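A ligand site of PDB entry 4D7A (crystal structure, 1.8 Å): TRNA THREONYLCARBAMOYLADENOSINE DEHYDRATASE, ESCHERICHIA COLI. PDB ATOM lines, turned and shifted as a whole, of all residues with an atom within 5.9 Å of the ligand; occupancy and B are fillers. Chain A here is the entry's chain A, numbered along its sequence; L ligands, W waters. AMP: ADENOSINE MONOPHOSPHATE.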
ATOM      1  N   VAL A  36     -21.983 -16.221 -16.990  1.00  0.00           N
ATOM      2  CA  VAL A  36     -21.039 -16.212 -18.105  1.00  0.00           C
ATOM      3  C   VAL A  36     -20.899 -14.784 -18.619  1.00  0.00           C
ATOM      4  O   VAL A  36     -21.851 -14.230 -19.147  1.00  0.00           O
ATOM      5  CB  VAL A  36     -21.481 -17.166 -19.249  1.00  0.00           C
ATOM      6  CG1 VAL A  36     -20.361 -17.299 -20.267  1.00  0.00           C
ATOM      7  CG2 VAL A  36     -21.850 -18.547 -18.692  1.00  0.00           C
ATOM      8  N   GLY A  37     -19.703 -14.207 -18.461  1.00  0.00           N
ATOM      9  CA  GLY A  37     -19.444 -12.825 -18.816  1.00  0.00           C
ATOM     10  C   GLY A  37     -19.582 -11.969 -17.568  1.00  0.00           C
ATOM     11  O   GLY A  37     -20.667 -11.851 -17.010  1.00  0.00           O
ATOM     12  N   ILE A  38     -18.471 -11.419 -17.090  1.00  0.00           N
ATOM     13  CA  ILE A  38     -18.467 -10.653 -15.844  1.00  0.00           C
ATOM     14  C   ILE A  38     -18.180  -9.166 -16.153  1.00  0.00           C
ATOM     15  O   ILE A  38     -17.248  -8.565 -15.626  1.00  0.00           O
ATOM     16  CB  ILE A  38     -17.423 -11.238 -14.862  1.00  0.00           C
ATOM     17  CG1 ILE A  38     -17.552 -12.762 -14.805  1.00  0.00           C
ATOM     18  CG2 ILE A  38     -17.622 -10.662 -13.459  1.00  0.00           C
ATOM     19  CD1 ILE A  38     -18.933 -13.278 -14.364  1.00  0.00           C
ATOM     20  N   GLY A  39     -18.987  -8.602 -17.042  1.00  0.00           N
ATOM     21  CA  GLY A  39     -18.780  -7.249 -17.517  1.00  0.00           C
ATOM     22  C   GLY A  39     -19.852  -6.302 -17.016  1.00  0.00           C
ATOM     23  O   GLY A  39     -20.257  -6.388 -15.857  1.00  0.00           O
ATOM     24  N   GLY A  40     -20.310  -5.424 -17.897  1.00  0.00           N
ATOM     25  CA  GLY A  40     -21.286  -4.394 -17.543  1.00  0.00           C
ATOM     26  C   GLY A  40     -22.586  -4.931 -16.984  1.00  0.00           C
ATOM     27  O   GLY A  40     -23.263  -4.278 -16.158  1.00  0.00           O
ATOM     28  N   VAL A  41     -22.974  -6.113 -17.457  1.00  0.00           N
ATOM     29  CA  VAL A  41     -24.168  -6.796 -16.956  1.00  0.00           C
ATOM     30  C   VAL A  41     -23.841  -7.865 -15.921  1.00  0.00           C
ATOM     31  O   VAL A  41     -24.404  -7.888 -14.826  1.00  0.00           O
ATOM     32  CB  VAL A  41     -24.973  -7.449 -18.121  1.00  0.00           C
ATOM     33  CG1 VAL A  41     -26.136  -8.301 -17.582  1.00  0.00           C
ATOM     34  CG2 VAL A  41     -25.496  -6.358 -19.049  1.00  0.00           C
ATOM     35  N   ILE A  60     -17.553 -17.163 -15.316  1.00  0.00           N
ATOM     36  CA  ILE A  60     -16.760 -17.498 -16.502  1.00  0.00           C
ATOM     37  C   ILE A  60     -16.391 -16.260 -17.303  1.00  0.00           C
ATOM     38  O   ILE A  60     -17.266 -15.587 -17.849  1.00  0.00           O
ATOM     39  CB  ILE A  60     -17.505 -18.496 -17.408  1.00  0.00           C
ATOM     40  CG1 ILE A  60     -17.963 -19.710 -16.591  1.00  0.00           C
ATOM     41  CG2 ILE A  60     -16.603 -18.950 -18.568  1.00  0.00           C
ATOM     42  CD1 ILE A  60     -18.552 -20.860 -17.411  1.00  0.00           C
ATOM     43  N   ASP A  61     -15.102 -15.928 -17.354  1.00  0.00           N
ATOM     44  CA  ASP A  61     -14.598 -14.786 -18.121  1.00  0.00           C
ATOM     45  C   ASP A  61     -13.085 -14.882 -18.187  1.00  0.00           C
ATOM     46  O   ASP A  61     -12.462 -15.359 -17.233  1.00  0.00           O
ATOM     47  CB  ASP A  61     -15.020 -13.448 -17.470  1.00  0.00           C
ATOM     48  CG  ASP A  61     -15.117 -12.289 -18.461  1.00  0.00           C
ATOM     49  OD1 ASP A  61     -14.309 -12.187 -19.409  1.00  0.00           O
ATOM     50  OD2 ASP A  61     -16.015 -11.445 -18.282  1.00  0.00           O
ATOM     51  N   MET A  62     -12.494 -14.444 -19.281  1.00  0.00           N
ATOM     52  CA  MET A  62     -11.039 -14.479 -19.401  1.00  0.00           C
ATOM     53  C   MET A  62     -10.429 -13.072 -19.437  1.00  0.00           C
ATOM     54  O   MET A  62      -9.208 -12.914 -19.495  1.00  0.00           O
ATOM     55  CB  MET A  62     -10.667 -15.272 -20.664  1.00  0.00           C
ATOM     56  CG  MET A  62      -9.297 -15.878 -20.659  1.00  0.00           C
ATOM     57  SD  MET A  62      -9.016 -16.766 -22.202  1.00  0.00           S
ATOM     58  CE  MET A  62      -7.240 -16.591 -22.361  1.00  0.00           C
ATOM     59  N   ASP A  63     -11.266 -12.044 -19.395  1.00  0.00           N
ATOM     60  CA  ASP A  63     -10.788 -10.657 -19.503  1.00  0.00           C
ATOM     61  C   ASP A  63     -10.223 -10.076 -18.210  1.00  0.00           C
ATOM     62  O   ASP A  63     -10.563 -10.525 -17.112  1.00  0.00           O
ATOM     63  CB  ASP A  63     -11.910  -9.750 -20.007  1.00  0.00           C
ATOM     64  CG  ASP A  63     -12.038  -9.766 -21.518  1.00  0.00           C
ATOM     65  OD1 ASP A  63     -11.284 -10.522 -22.170  1.00  0.00           O
ATOM     66  OD2 ASP A  63     -12.874  -9.014 -22.054  1.00  0.00           O
ATOM     67  N   ASN A  69     -13.460   0.171 -17.951  1.00  0.00           N
ATOM     68  CA  ASN A  69     -14.619  -0.512 -17.367  1.00  0.00           C
ATOM     69  C   ASN A  69     -15.344   0.315 -16.310  1.00  0.00           C
ATOM     70  O   ASN A  69     -16.434  -0.035 -15.872  1.00  0.00           O
ATOM     71  CB  ASN A  69     -14.240  -1.838 -16.671  1.00  0.00           C
ATOM     72  CG  ASN A  69     -13.580  -2.871 -17.593  1.00  0.00           C
ATOM     73  OD1 ASN A  69     -12.914  -3.779 -17.111  1.00  0.00           O
ATOM     74  ND2 ASN A  69     -13.784  -2.759 -18.901  1.00  0.00           N
ATOM     75  N   ARG A  72     -19.176   1.227 -15.727  1.00  0.00           N
ATOM     76  CA  ARG A  72     -20.283   0.262 -15.717  1.00  0.00           C
ATOM     77  C   ARG A  72     -20.046  -1.115 -15.076  1.00  0.00           C
ATOM     78  O   ARG A  72     -20.901  -1.987 -15.186  1.00  0.00           O
ATOM     79  CB  ARG A  72     -20.745   0.027 -17.146  1.00  0.00           C
ATOM     80  CG  ARG A  72     -19.689  -0.725 -18.000  1.00  0.00           C
ATOM     81  CD  ARG A  72     -19.915  -0.551 -19.496  1.00  0.00           C
ATOM     82  NE  ARG A  72     -19.038  -1.412 -20.290  1.00  0.00           N
ATOM     83  CZ  ARG A  72     -17.776  -1.126 -20.587  1.00  0.00           C
ATOM     84  NH1 ARG A  72     -17.231   0.002 -20.140  1.00  0.00           N
ATOM     85  NH2 ARG A  72     -17.051  -1.974 -21.311  1.00  0.00           N
ATOM     86  N   GLN A  73     -18.893  -1.328 -14.428  1.00  0.00           N
ATOM     87  CA  GLN A  73     -18.575  -2.661 -13.879  1.00  0.00           C
ATOM     88  C   GLN A  73     -18.153  -2.559 -12.416  1.00  0.00           C
ATOM     89  O   GLN A  73     -17.292  -1.741 -12.066  1.00  0.00           O
ATOM     90  CB  GLN A  73     -17.495  -3.340 -14.740  1.00  0.00           C
ATOM     91  CG  GLN A  73     -17.863  -3.322 -16.230  1.00  0.00           C
ATOM     92  CD  GLN A  73     -16.957  -4.123 -17.145  1.00  0.00           C
ATOM     93  OE1 GLN A  73     -16.211  -4.995 -16.713  1.00  0.00           O
ATOM     94  NE2 GLN A  73     -17.044  -3.833 -18.440  1.00  0.00           N
ATOM     95  N   LYS A  85     -10.910 -10.167 -14.142  1.00  0.00           N
ATOM     96  CA  LYS A  85     -12.241  -9.762 -13.680  1.00  0.00           C
ATOM     97  C   LYS A  85     -12.884 -10.837 -12.812  1.00  0.00           C
ATOM     98  O   LYS A  85     -13.446 -10.556 -11.750  1.00  0.00           O
ATOM     99  CB  LYS A  85     -13.168  -9.500 -14.864  1.00  0.00           C
ATOM    100  CG  LYS A  85     -12.867  -8.284 -15.686  1.00  0.00           C
ATOM    101  CD  LYS A  85     -13.892  -8.188 -16.808  1.00  0.00           C
ATOM    102  CE  LYS A  85     -13.670  -6.968 -17.663  1.00  0.00           C
ATOM    103  NZ  LYS A  85     -14.731  -6.824 -18.683  1.00  0.00           N
ATOM    104  N   ASP A 107     -11.694 -18.546 -18.944  1.00  0.00           N
ATOM    105  CA  ASP A 107     -11.835 -18.983 -20.319  1.00  0.00           C
ATOM    106  C   ASP A 107     -13.010 -18.255 -20.956  1.00  0.00           C
ATOM    107  O   ASP A 107     -13.786 -17.599 -20.263  1.00  0.00           O
ATOM    108  CB  ASP A 107     -12.044 -20.495 -20.385  1.00  0.00           C
ATOM    109  CG  ASP A 107     -11.613 -21.098 -21.704  1.00  0.00           C
ATOM    110  OD1 ASP A 107     -11.170 -20.331 -22.593  1.00  0.00           O
ATOM    111  OD2 ASP A 107     -11.710 -22.331 -21.858  1.00  0.00           O
ATOM    112  N   PHE A 108     -13.132 -18.372 -22.272  1.00  0.00           N
ATOM    113  CA  PHE A 108     -14.325 -17.918 -22.972  1.00  0.00           C
ATOM    114  C   PHE A 108     -15.085 -19.139 -23.450  1.00  0.00           C
ATOM    115  O   PHE A 108     -14.476 -20.153 -23.784  1.00  0.00           O
ATOM    116  CB  PHE A 108     -13.975 -17.027 -24.180  1.00  0.00           C
ATOM    117  CG  PHE A 108     -13.333 -15.722 -23.821  1.00  0.00           C
ATOM    118  CD1 PHE A 108     -13.934 -14.848 -22.920  1.00  0.00           C
ATOM    119  CD2 PHE A 108     -12.116 -15.352 -24.381  1.00  0.00           C
ATOM    120  CE1 PHE A 108     -13.350 -13.634 -22.600  1.00  0.00           C
ATOM    121  CE2 PHE A 108     -11.516 -14.151 -24.052  1.00  0.00           C
ATOM    122  CZ  PHE A 108     -12.136 -13.296 -23.166  1.00  0.00           C
ATOM    123  N   VAL A 109     -16.405 -19.042 -23.495  1.00  0.00           N
ATOM    124  CA  VAL A 109     -17.232 -20.145 -23.985  1.00  0.00           C
ATOM    125  C   VAL A 109     -17.153 -20.202 -25.511  1.00  0.00           C
ATOM    126  O   VAL A 109     -17.240 -19.188 -26.186  1.00  0.00           O
ATOM    127  CB  VAL A 109     -18.697 -20.005 -23.544  1.00  0.00           C
ATOM    128  CG1 VAL A 109     -19.559 -21.103 -24.178  1.00  0.00           C
ATOM    129  CG2 VAL A 109     -18.783 -20.101 -22.026  1.00  0.00           C
ATOM    130  N   THR A 110     -16.952 -21.403 -26.024  1.00  0.00           N
ATOM    131  CA  THR A 110     -16.977 -21.650 -27.460  1.00  0.00           C
ATOM    132  C   THR A 110     -17.893 -22.840 -27.720  1.00  0.00           C
ATOM    133  O   THR A 110     -18.202 -23.594 -26.794  1.00  0.00           O
ATOM    134  CB  THR A 110     -15.551 -21.955 -28.013  1.00  0.00           C
ATOM    135  OG1 THR A 110     -15.157 -23.263 -27.590  1.00  0.00           O
ATOM    136  CG2 THR A 110     -14.549 -20.930 -27.514  1.00  0.00           C
ATOM    137  N   ALA A 128     -24.453 -13.453 -19.830  1.00  0.00           N
ATOM    138  CA  ALA A 128     -24.167 -12.022 -19.923  1.00  0.00           C
ATOM    139  C   ALA A 128     -23.015 -11.772 -20.893  1.00  0.00           C
ATOM    140  O   ALA A 128     -22.200 -10.877 -20.699  1.00  0.00           O
ATOM    141  CB  ALA A 128     -23.860 -11.443 -18.539  1.00  0.00           C
ATOM    142  N   ILE A 129     -22.979 -12.577 -21.948  1.00  0.00           N
ATOM    143  CA  ILE A 129     -21.949 -12.476 -22.994  1.00  0.00           C
ATOM    144  C   ILE A 129     -22.351 -11.384 -23.983  1.00  0.00           C
ATOM    145  O   ILE A 129     -23.513 -11.315 -24.370  1.00  0.00           O
ATOM    146  CB  ILE A 129     -21.771 -13.797 -23.780  1.00  0.00           C
ATOM    147  CG1 ILE A 129     -21.410 -14.959 -22.845  1.00  0.00           C
ATOM    148  CG2 ILE A 129     -20.732 -13.656 -24.886  1.00  0.00           C
ATOM    149  CD1 ILE A 129     -21.534 -16.326 -23.533  1.00  0.00           C
ATOM    150  N   ASP A 130     -21.397 -10.566 -24.417  1.00  0.00           N
ATOM    151  CA  ASP A 130     -21.749  -9.432 -25.264  1.00  0.00           C
ATOM    152  C   ASP A 130     -21.502  -9.679 -26.761  1.00  0.00           C
ATOM    153  O   ASP A 130     -21.843  -8.823 -27.581  1.00  0.00           O
ATOM    154  CB  ASP A 130     -20.972  -8.175 -24.810  1.00  0.00           C
ATOM    155  CG  ASP A 130     -19.467  -8.309 -24.986  1.00  0.00           C
ATOM    156  OD1 ASP A 130     -18.974  -9.407 -25.321  1.00  0.00           O
ATOM    157  OD2 ASP A 130     -18.760  -7.299 -24.789  1.00  0.00           O
ATOM    158  N   SER A 131     -20.944 -10.837 -27.112  1.00  0.00           N
ATOM    159  CA  SER A 131     -20.651 -11.155 -28.512  1.00  0.00           C
ATOM    160  C   SER A 131     -21.475 -12.329 -29.042  1.00  0.00           C
ATOM    161  O   SER A 131     -21.679 -13.310 -28.335  1.00  0.00           O
ATOM    162  CB  SER A 131     -19.153 -11.440 -28.678  1.00  0.00           C
ATOM    163  OG  SER A 131     -18.752 -12.565 -27.931  1.00  0.00           O
ATOM    164  N   PRO A 134     -20.295 -16.853 -29.449  1.00  0.00           N
ATOM    165  CA  PRO A 134     -20.379 -17.700 -28.251  1.00  0.00           C
ATOM    166  C   PRO A 134     -21.731 -17.625 -27.542  1.00  0.00           C
ATOM    167  O   PRO A 134     -22.126 -18.572 -26.871  1.00  0.00           O
ATOM    168  CB  PRO A 134     -19.287 -17.141 -27.347  1.00  0.00           C
ATOM    169  CG  PRO A 134     -19.086 -15.743 -27.801  1.00  0.00           C
ATOM    170  CD  PRO A 134     -19.330 -15.751 -29.271  1.00  0.00           C
ATOM    171  N   LYS A 135     -22.390 -16.485 -27.638  1.00  0.00           N
ATOM    172  CA  LYS A 135     -23.706 -16.304 -27.047  1.00  0.00           C
ATOM    173  C   LYS A 135     -24.694 -17.313 -27.648  1.00  0.00           C
ATOM    174  O   LYS A 135     -25.405 -17.997 -26.924  1.00  0.00           O
ATOM    175  CB  LYS A 135     -24.198 -14.865 -27.256  1.00  0.00           C
ATOM    176  CG  LYS A 135     -25.309 -14.434 -26.328  1.00  0.00           C
ATOM    177  CD  LYS A 135     -25.501 -12.906 -26.420  1.00  0.00           C
ATOM    178  CE  LYS A 135     -26.557 -12.409 -25.472  1.00  0.00           C
ATOM    179  NZ  LYS A 135     -26.115 -12.438 -24.054  1.00  0.00           N
HETATM  180  P   AMP L   1     -19.340  -5.451 -21.459  1.00  0.00           P
HETATM  181  O1P AMP L   1     -19.938  -4.560 -20.403  1.00  0.00           O
HETATM  182  O2P AMP L   1     -17.999  -4.910 -21.893  1.00  0.00           O
HETATM  183  O3P AMP L   1     -20.262  -5.787 -22.597  1.00  0.00           O
HETATM  184  O5' AMP L   1     -19.056  -6.866 -20.744  1.00  0.00           O
HETATM  185  C5' AMP L   1     -19.027  -8.095 -21.487  1.00  0.00           C
HETATM  186  C4' AMP L   1     -18.206  -9.156 -20.795  1.00  0.00           C
HETATM  187  O4' AMP L   1     -18.451 -10.477 -21.378  1.00  0.00           O
HETATM  188  C3' AMP L   1     -16.679  -8.939 -20.859  1.00  0.00           C
HETATM  189  O3' AMP L   1     -16.111  -9.046 -19.546  1.00  0.00           O
HETATM  190  C2' AMP L   1     -16.180 -10.107 -21.732  1.00  0.00           C
HETATM  191  O2' AMP L   1     -14.870 -10.549 -21.454  1.00  0.00           O
HETATM  192  C1' AMP L   1     -17.217 -11.179 -21.449  1.00  0.00           C
HETATM  193  N9  AMP L   1     -17.275 -12.228 -22.486  1.00  0.00           N
HETATM  194  C8  AMP L   1     -17.264 -11.976 -23.812  1.00  0.00           C
HETATM  195  N7  AMP L   1     -17.275 -13.126 -24.548  1.00  0.00           N
HETATM  196  C5  AMP L   1     -17.281 -14.154 -23.679  1.00  0.00           C
HETATM  197  C6  AMP L   1     -17.301 -15.638 -23.796  1.00  0.00           C
HETATM  198  N6  AMP L   1     -17.314 -16.232 -25.009  1.00  0.00           N
HETATM  199  N1  AMP L   1     -17.301 -16.368 -22.658  1.00  0.00           N
HETATM  200  C2  AMP L   1     -17.279 -15.785 -21.443  1.00  0.00           C
HETATM  201  N3  AMP L   1     -17.253 -14.449 -21.269  1.00  0.00           N
HETATM  202  C4  AMP L   1     -17.253 -13.572 -22.316  1.00  0.00           C
HETATM  203  O   HOH W   1     -15.830  -5.278 -20.624  1.00  0.00           O
HETATM  204  O   HOH W   2     -21.981  -6.912 -20.260  1.00  0.00           O
HETATM  205  O   HOH W   3     -15.557 -14.572 -27.243  1.00  0.00           O
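Water W1 lies within hydrogen-bond range of O2P of the ligand (2.5 Å), NZ of Lys 85 (2.7 Å) and NE2 of Gln 73 (2.9 Å).
Water W2 lies within hydrogen-bond range of O5' of the ligand (3.0 Å), N of Val 41 (3.1 Å) and N of Gly 40 (3.3 Å).
The backbone NH (N) of Ala 128 is in hydrogen-bond range of the backbone carbonyl oxygen (O) of Val 36 (2.8 Å).
N of Ile 129 lies within hydrogen-bond range of O of Val 36, 3.4 Å away.
OE1 of Gln 73 lies within hydrogen-bond range of NZ of Lys 85 (3.1 Å).
The backbone carbonyl oxygen of Ile 60 lies within hydrogen-bond range of the backbone NH of Gly 37 (2.9 Å).
N of Asp 63 lies within hydrogen-bond range of OD1 of Asp 61 (3.0 Å).
The side-chain carboxylate (OD2) of Asp 61 lies within hydrogen-bond range of the backbone NH (N) of Ile 38, at 2.7 Å.
The side-chain amide nitrogen (NE2) of Gln 73 lies close to the side-chain amide nitrogen (ND2) of Asn 69 (3.5 Å).
NH2 of Arg 72 sits close to NE2 of Gln 73 (3.4 Å).
The guanidinium group of Arg 72 is in salt-bridge range of an oxygen (O2P) of the ligand (3.1 Å).
The side-chain carboxylate of Asp 130 lies close to an oxygen (O3P) of the ligand (3.1 Å).
OD1 of Asp 61 lies within hydrogen-bond range of O2' of the ligand, at 2.7 Å.
N6 of the ligand sits at hydrogen-bond distance from O of Val 109.
O2' of the ligand sits at hydrogen-bond distance from OD2 of Asp 63 (2.6 Å).
N of Val 109 is in hydrogen-bond range of N1 of the ligand (2.9 Å).
An oxygen (O3') of the ligand is in hydrogen-bond range of the side-chain amino group (NZ) of Lys 85 (2.8 Å).
N of Gly 40 sits at hydrogen-bond distance from O1P of the ligand (2.7 Å).
Val 36 touches the ligand.
Gly 37 touches the ligand.
C of Ile 38 touches O3' of the ligand (3.98 Å).
CA of Gly 39 touches O5' of the ligand, at 3.3 Å.
Ile 60 touches the ligand.
NE2 of Gln 73 touches O1P of the ligand, 3.6 Å away.
Phe 108 touches the ligand.
Ala 128 touches the ligand (O to O4', 3.8 Å).
Ile 129 touches the ligand.
Ser 131 touches the ligand.
Pro 134 touches the ligand.
Hydrophobic or aromatic side chains within 4 Å of the ligand: Val 36, Phe 108, Val 109, Ile 129 and Pro 134.
18 residues have an atom within 4 Å of the ligand: Val 36, Gly 37, Ile 38, Gly 39, Gly 40, Ile 60, Asp 61, Asp 63, Arg 72, Gln 73, Lys 85, Phe 108, Val 109, Ala 128, Ile 129, Asp 130, Ser 131 and Pro 134.
Along chain A the residues within 4 Å of the ligand span positions 36 to 134.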
